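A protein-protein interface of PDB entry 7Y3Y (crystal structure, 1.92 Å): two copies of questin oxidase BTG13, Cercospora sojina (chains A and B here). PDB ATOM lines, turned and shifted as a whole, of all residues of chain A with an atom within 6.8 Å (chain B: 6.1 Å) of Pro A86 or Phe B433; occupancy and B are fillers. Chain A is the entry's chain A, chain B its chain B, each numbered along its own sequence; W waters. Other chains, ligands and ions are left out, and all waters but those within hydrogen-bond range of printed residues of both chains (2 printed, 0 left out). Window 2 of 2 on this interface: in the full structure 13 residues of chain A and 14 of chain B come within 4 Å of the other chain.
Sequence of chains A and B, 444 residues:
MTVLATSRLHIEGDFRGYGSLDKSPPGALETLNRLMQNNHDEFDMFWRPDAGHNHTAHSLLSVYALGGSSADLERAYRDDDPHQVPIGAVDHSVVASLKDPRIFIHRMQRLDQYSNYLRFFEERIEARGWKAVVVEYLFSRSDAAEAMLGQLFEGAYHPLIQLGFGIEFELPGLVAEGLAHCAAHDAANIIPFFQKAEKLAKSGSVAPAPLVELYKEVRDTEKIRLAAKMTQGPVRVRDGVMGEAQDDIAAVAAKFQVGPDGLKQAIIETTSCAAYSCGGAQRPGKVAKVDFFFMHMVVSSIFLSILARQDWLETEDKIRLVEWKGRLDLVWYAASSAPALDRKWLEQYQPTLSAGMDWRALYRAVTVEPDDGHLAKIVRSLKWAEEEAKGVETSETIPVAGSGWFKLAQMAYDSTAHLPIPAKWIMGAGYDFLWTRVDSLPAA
The side-chain carboxylate of Asp A81 is in salt-bridge range of the guanidinium group of Arg B437 (3.8 Å).
O of Gln A84 sits at hydrogen-bond distance from NH2 of Arg B437 (3.1 Å).
The backbone NH (N) of Asp A44 is in hydrogen-bond range of the backbone carbonyl oxygen (O) of Val A85, 2.9 Å away.
OG1 of Thr B436 lies within hydrogen-bond range of O of Phe B433, 2.6 Å away.
Gln A84 touches Phe B433 (O to CZ, 3.3 Å).
Val A85 touches Met B230.
Thr B231 touches Val A85.
CG of Pro A86 touches CD1 of Phe B433, 3.6 Å away.
Pro A86 touches just one residue of chain B: Phe B433 (3.6 Å).
Of the printed residues of chain A, Met B230 touches Val A85 (3.97 Å).
Printed residues of chain B within 4 Å of Gln A84: Phe B433 and Arg B437.
Asp B432 touches none of the printed residues of chain A.
The nearest residue of chain B that does not touch Pro A86 is Met B230 (4.3 Å).
The nearest printed residue of chain B that does not touch Asp A81 is Phe B433 (5.7 Å).
Hydrophobic or aromatic side chains of chain A within 4 Å of the printed part of chain B: Val A85 and Pro A86.
Among the printed residues, Asp or Glu carboxylates within 4 Å of a Lys or Arg side-chain nitrogen of the other chain: Asp A81 with Arg B437.
No position is printed for both chains.
Water W1 bridges OD1 of Asp A81 and NE of Arg B437.
Water W2 bridges OG1 of Thr B231 (2.8 Å) and O of Phe A46 (2.9 Å).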
ATOM      1  N   GLU A  42      15.669  -8.025  15.948  1.00  0.00           N
ATOM      2  CA  GLU A  42      16.126  -8.450  14.605  1.00  0.00           C
ATOM      3  C   GLU A  42      16.673  -7.244  13.829  1.00  0.00           C
ATOM      4  O   GLU A  42      17.567  -7.445  13.002  1.00  0.00           O
ATOM      5  CB  GLU A  42      14.989  -9.092  13.807  1.00  0.00           C
ATOM      6  CG  GLU A  42      14.521 -10.442  14.325  1.00  0.00           C
ATOM      7  CD  GLU A  42      13.253 -11.014  13.668  1.00  0.00           C
ATOM      8  OE1 GLU A  42      13.110 -10.892  12.405  1.00  0.00           O
ATOM      9  OE2 GLU A  42      12.378 -11.598  14.422  1.00  0.00           O
ATOM     10  N   PHE A  43      16.144  -6.030  14.032  1.00  0.00           N
ATOM     11  CA  PHE A  43      16.329  -4.940  13.030  1.00  0.00           C
ATOM     12  C   PHE A  43      17.067  -3.723  13.605  1.00  0.00           C
ATOM     13  O   PHE A  43      16.935  -3.377  14.777  1.00  0.00           O
ATOM     14  CB  PHE A  43      14.998  -4.542  12.407  1.00  0.00           C
ATOM     15  CG  PHE A  43      14.255  -5.697  11.772  1.00  0.00           C
ATOM     16  CD1 PHE A  43      14.896  -6.577  10.919  1.00  0.00           C
ATOM     17  CD2 PHE A  43      12.906  -5.915  12.041  1.00  0.00           C
ATOM     18  CE1 PHE A  43      14.203  -7.641  10.352  1.00  0.00           C
ATOM     19  CE2 PHE A  43      12.207  -6.960  11.449  1.00  0.00           C
ATOM     20  CZ  PHE A  43      12.864  -7.828  10.607  1.00  0.00           C
ATOM     21  N   ASP A  44      17.790  -3.041  12.720  1.00  0.00           N
ATOM     22  CA  ASP A  44      18.501  -1.806  13.071  1.00  0.00           C
ATOM     23  C   ASP A  44      17.498  -0.672  13.188  1.00  0.00           C
ATOM     24  O   ASP A  44      16.359  -0.811  12.734  1.00  0.00           O
ATOM     25  CB  ASP A  44      19.598  -1.497  12.067  1.00  0.00           C
ATOM     26  CG  ASP A  44      20.759  -0.782  12.720  1.00  0.00           C
ATOM     27  OD1 ASP A  44      21.683  -1.495  13.205  1.00  0.00           O
ATOM     28  OD2 ASP A  44      20.733   0.475  12.758  1.00  0.00           O
ATOM     29  N   PHE A  46      18.439   2.177  11.753  1.00  0.00           N
ATOM     30  CA  PHE A  46      18.721   2.945  10.519  1.00  0.00           C
ATOM     31  C   PHE A  46      18.924   1.988   9.354  1.00  0.00           C
ATOM     32  O   PHE A  46      19.755   1.076   9.450  1.00  0.00           O
ATOM     33  CB  PHE A  46      19.892   3.883  10.747  1.00  0.00           C
ATOM     34  CG  PHE A  46      19.816   4.699  12.012  1.00  0.00           C
ATOM     35  CD1 PHE A  46      19.055   5.840  12.052  1.00  0.00           C
ATOM     36  CD2 PHE A  46      20.631   4.414  13.102  1.00  0.00           C
ATOM     37  CE1 PHE A  46      19.032   6.635  13.183  1.00  0.00           C
ATOM     38  CE2 PHE A  46      20.613   5.203  14.239  1.00  0.00           C
ATOM     39  CZ  PHE A  46      19.813   6.318  14.263  1.00  0.00           C
ATOM     40  N   ASP A  81       8.283  -3.348   5.986  1.00  0.00           N
ATOM     41  CA  ASP A  81       9.337  -4.297   5.535  1.00  0.00           C
ATOM     42  C   ASP A  81      10.579  -3.531   5.047  1.00  0.00           C
ATOM     43  O   ASP A  81      11.704  -3.897   5.412  1.00  0.00           O
ATOM     44  CB  ASP A  81       8.821  -5.273   4.472  1.00  0.00           C
ATOM     45  CG  ASP A  81       9.897  -6.294   4.136  1.00  0.00           C
ATOM     46  OD1 ASP A  81      10.178  -7.109   4.981  1.00  0.00           O
ATOM     47  OD2 ASP A  81      10.461  -6.226   3.054  1.00  0.00           O
ATOM     48  N   GLN A  84      13.155  -2.478   7.595  1.00  0.00           N
ATOM     49  CA  GLN A  84      13.599  -3.570   8.485  1.00  0.00           C
ATOM     50  C   GLN A  84      14.854  -4.225   7.894  1.00  0.00           C
ATOM     51  O   GLN A  84      14.748  -4.988   6.923  1.00  0.00           O
ATOM     52  CB  GLN A  84      12.472  -4.569   8.679  1.00  0.00           C
ATOM     53  CG  GLN A  84      11.326  -3.996   9.486  1.00  0.00           C
ATOM     54  CD  GLN A  84      10.036  -4.747   9.356  1.00  0.00           C
ATOM     55  OE1 GLN A  84       9.942  -5.821   8.718  1.00  0.00           O
ATOM     56  NE2 GLN A  84       9.017  -4.147   9.946  1.00  0.00           N
ATOM     57  N   VAL A  85      16.018  -3.876   8.414  1.00  0.00           N
ATOM     58  CA  VAL A  85      17.308  -4.508   7.987  1.00  0.00           C
ATOM     59  C   VAL A  85      18.008  -5.059   9.218  1.00  0.00           C
ATOM     60  O   VAL A  85      17.731  -4.638  10.325  1.00  0.00           O
ATOM     61  CB  VAL A  85      18.219  -3.537   7.230  1.00  0.00           C
ATOM     62  CG1 VAL A  85      17.511  -2.928   6.039  1.00  0.00           C
ATOM     63  CG2 VAL A  85      18.761  -2.469   8.157  1.00  0.00           C
ATOM     64  N   PRO A  86      18.931  -6.026   9.066  1.00  0.00           N
ATOM     65  CA  PRO A  86      19.577  -6.679  10.213  1.00  0.00           C
ATOM     66  C   PRO A  86      20.306  -5.701  11.132  1.00  0.00           C
ATOM     67  O   PRO A  86      21.034  -4.858  10.643  1.00  0.00           O
ATOM     68  CB  PRO A  86      20.574  -7.665   9.567  1.00  0.00           C
ATOM     69  CG  PRO A  86      19.913  -7.950   8.217  1.00  0.00           C
ATOM     70  CD  PRO A  86      19.399  -6.589   7.788  1.00  0.00           C
ATOM     71  N   ILE A  87      20.012  -5.805  12.430  1.00  0.00           N
ATOM     72  CA  ILE A  87      20.679  -5.025  13.504  1.00  0.00           C
ATOM     73  C   ILE A  87      22.191  -5.320  13.487  1.00  0.00           C
ATOM     74  O   ILE A  87      22.589  -6.476  13.238  1.00  0.00           O
ATOM     75  CB  ILE A  87      20.056  -5.312  14.885  1.00  0.00           C
ATOM     76  CG1 ILE A  87      20.549  -4.299  15.915  1.00  0.00           C
ATOM     77  CG2 ILE A  87      20.266  -6.757  15.357  1.00  0.00           C
ATOM     78  CD1 ILE A  87      19.656  -4.214  17.111  1.00  0.00           C
ATOM     79  N   GLY A  88      22.984  -4.276  13.681  1.00  0.00           N
ATOM     80  CA  GLY A  88      24.449  -4.354  13.648  1.00  0.00           C
ATOM     81  C   GLY A  88      24.952  -5.233  14.764  1.00  0.00           C
ATOM     82  O   GLY A  88      24.283  -5.314  15.811  1.00  0.00           O
ATOM     83  N   ALA A  89      26.039  -5.953  14.479  1.00  0.00           N
ATOM     84  CA  ALA A  89      26.798  -6.754  15.458  1.00  0.00           C
ATOM     85  C   ALA A  89      27.175  -5.805  16.594  1.00  0.00           C
ATOM     86  O   ALA A  89      27.546  -4.687  16.281  1.00  0.00           O
ATOM     87  CB  ALA A  89      28.000  -7.373  14.771  1.00  0.00           C
ATOM     88  N   MET B 230      26.300  -2.543   4.178  1.00  0.00           N
ATOM     89  CA  MET B 230      25.077  -2.551   3.349  1.00  0.00           C
ATOM     90  C   MET B 230      24.389  -1.193   3.494  1.00  0.00           C
ATOM     91  O   MET B 230      24.047  -0.584   2.467  1.00  0.00           O
ATOM     92  CB  MET B 230      24.101  -3.655   3.770  1.00  0.00           C
ATOM     93  CG  MET B 230      23.043  -3.907   2.705  1.00  0.00           C
ATOM     94  SD  MET B 230      21.832  -5.167   3.187  1.00  0.00           S
ATOM     95  CE  MET B 230      21.020  -4.320   4.531  1.00  0.00           C
ATOM     96  N   THR B 231      24.186  -0.746   4.728  1.00  0.00           N
ATOM     97  CA  THR B 231      23.314   0.427   5.017  1.00  0.00           C
ATOM     98  C   THR B 231      24.082   1.752   4.853  1.00  0.00           C
ATOM     99  O   THR B 231      23.463   2.836   5.087  1.00  0.00           O
ATOM    100  CB  THR B 231      22.657   0.317   6.393  1.00  0.00           C
ATOM    101  OG1 THR B 231      23.724   0.321   7.337  1.00  0.00           O
ATOM    102  CG2 THR B 231      21.752  -0.877   6.492  1.00  0.00           C
ATOM    103  N   TYR B 431      25.809  -8.664  -0.447  1.00  0.00           N
ATOM    104  CA  TYR B 431      25.096  -8.604   0.843  1.00  0.00           C
ATOM    105  C   TYR B 431      23.972  -9.646   0.838  1.00  0.00           C
ATOM    106  O   TYR B 431      22.931  -9.468   0.113  1.00  0.00           O
ATOM    107  CB  TYR B 431      24.624  -7.189   1.110  1.00  0.00           C
ATOM    108  CG  TYR B 431      25.715  -6.151   1.065  1.00  0.00           C
ATOM    109  CD1 TYR B 431      26.587  -6.001   2.136  1.00  0.00           C
ATOM    110  CD2 TYR B 431      25.830  -5.261  -0.011  1.00  0.00           C
ATOM    111  CE1 TYR B 431      27.566  -5.018   2.136  1.00  0.00           C
ATOM    112  CE2 TYR B 431      26.824  -4.278  -0.032  1.00  0.00           C
ATOM    113  CZ  TYR B 431      27.707  -4.175   1.038  1.00  0.00           C
ATOM    114  OH  TYR B 431      28.701  -3.241   1.051  1.00  0.00           O
ATOM    115  N   ASP B 432      24.117 -10.663   1.701  1.00  0.00           N
ATOM    116  CA  ASP B 432      23.154 -11.800   1.733  1.00  0.00           C
ATOM    117  C   ASP B 432      21.749 -11.253   1.945  1.00  0.00           C
ATOM    118  O   ASP B 432      20.816 -11.712   1.274  1.00  0.00           O
ATOM    119  CB  ASP B 432      23.399 -12.802   2.862  1.00  0.00           C
ATOM    120  CG  ASP B 432      24.719 -13.503   2.740  1.00  0.00           C
ATOM    121  OD1 ASP B 432      25.235 -13.551   1.618  1.00  0.00           O
ATOM    122  OD2 ASP B 432      25.219 -13.947   3.778  1.00  0.00           O
ATOM    123  N   PHE B 433      21.609 -10.251   2.795  1.00  0.00           N
ATOM    124  CA  PHE B 433      20.242  -9.838   3.175  1.00  0.00           C
ATOM    125  C   PHE B 433      19.472  -9.363   1.937  1.00  0.00           C
ATOM    126  O   PHE B 433      18.240  -9.563   1.944  1.00  0.00           O
ATOM    127  CB  PHE B 433      20.263  -8.758   4.250  1.00  0.00           C
ATOM    128  CG  PHE B 433      18.893  -8.197   4.506  1.00  0.00           C
ATOM    129  CD1 PHE B 433      17.990  -8.877   5.325  1.00  0.00           C
ATOM    130  CD2 PHE B 433      18.502  -7.010   3.904  1.00  0.00           C
ATOM    131  CE1 PHE B 433      16.724  -8.352   5.557  1.00  0.00           C
ATOM    132  CE2 PHE B 433      17.228  -6.505   4.127  1.00  0.00           C
ATOM    133  CZ  PHE B 433      16.359  -7.163   4.973  1.00  0.00           C
ATOM    134  N   LEU B 434      20.134  -8.753   0.933  1.00  0.00           N
ATOM    135  CA  LEU B 434      19.398  -8.216  -0.250  1.00  0.00           C
ATOM    136  C   LEU B 434      18.784  -9.384  -1.040  1.00  0.00           C
ATOM    137  O   LEU B 434      17.764  -9.151  -1.697  1.00  0.00           O
ATOM    138  CB  LEU B 434      20.303  -7.325  -1.115  1.00  0.00           C
ATOM    139  CG  LEU B 434      20.794  -6.051  -0.423  1.00  0.00           C
ATOM    140  CD1 LEU B 434      21.729  -5.250  -1.316  1.00  0.00           C
ATOM    141  CD2 LEU B 434      19.618  -5.174   0.036  1.00  0.00           C
ATOM    142  N   TRP B 435      19.343 -10.586  -0.971  1.00  0.00           N
ATOM    143  CA  TRP B 435      18.780 -11.775  -1.677  1.00  0.00           C
ATOM    144  C   TRP B 435      17.520 -12.319  -0.982  1.00  0.00           C
ATOM    145  O   TRP B 435      16.807 -13.095  -1.652  1.00  0.00           O
ATOM    146  CB  TRP B 435      19.825 -12.879  -1.875  1.00  0.00           C
ATOM    147  CG  TRP B 435      20.873 -12.486  -2.871  1.00  0.00           C
ATOM    148  CD1 TRP B 435      22.069 -11.882  -2.603  1.00  0.00           C
ATOM    149  CD2 TRP B 435      20.790 -12.572  -4.301  1.00  0.00           C
ATOM    150  NE1 TRP B 435      22.761 -11.633  -3.758  1.00  0.00           N
ATOM    151  CE2 TRP B 435      21.993 -12.024  -4.820  1.00  0.00           C
ATOM    152  CE3 TRP B 435      19.828 -13.057  -5.194  1.00  0.00           C
ATOM    153  CZ2 TRP B 435      22.260 -11.958  -6.184  1.00  0.00           C
ATOM    154  CZ3 TRP B 435      20.101 -13.004  -6.544  1.00  0.00           C
ATOM    155  CH2 TRP B 435      21.290 -12.452  -7.030  1.00  0.00           C
ATOM    156  N   THR B 436      17.234 -11.958   0.275  1.00  0.00           N
ATOM    157  CA  THR B 436      15.958 -12.356   0.942  1.00  0.00           C
ATOM    158  C   THR B 436      14.790 -11.582   0.317  1.00  0.00           C
ATOM    159  O   THR B 436      13.658 -12.034   0.465  1.00  0.00           O
ATOM    160  CB  THR B 436      15.975 -12.156   2.465  1.00  0.00           C
ATOM    161  OG1 THR B 436      16.049 -10.761   2.731  1.00  0.00           O
ATOM    162  CG2 THR B 436      17.127 -12.837   3.160  1.00  0.00           C
ATOM    163  N   ARG B 437      15.023 -10.468  -0.385  1.00  0.00           N
ATOM    164  CA  ARG B 437      13.919  -9.719  -1.060  1.00  0.00           C
ATOM    165  C   ARG B 437      13.814 -10.132  -2.551  1.00  0.00           C
ATOM    166  O   ARG B 437      12.982  -9.537  -3.272  1.00  0.00           O
ATOM    167  CB  ARG B 437      14.117  -8.210  -0.877  1.00  0.00           C
ATOM    168  CG  ARG B 437      13.868  -7.725   0.539  1.00  0.00           C
ATOM    169  CD  ARG B 437      14.378  -6.313   0.764  1.00  0.00           C
ATOM    170  NE  ARG B 437      14.104  -5.883   2.130  1.00  0.00           N
ATOM    171  CZ  ARG B 437      14.498  -4.717   2.647  1.00  0.00           C
ATOM    172  NH1 ARG B 437      15.188  -3.865   1.900  1.00  0.00           N
ATOM    173  NH2 ARG B 437      14.225  -4.419   3.914  1.00  0.00           N
HETATM  174  O   HOH W   1      12.768  -7.599   4.060  1.00  0.00           O
HETATM  175  O   HOH W   2      22.538   1.768   9.483  1.00  0.00           O
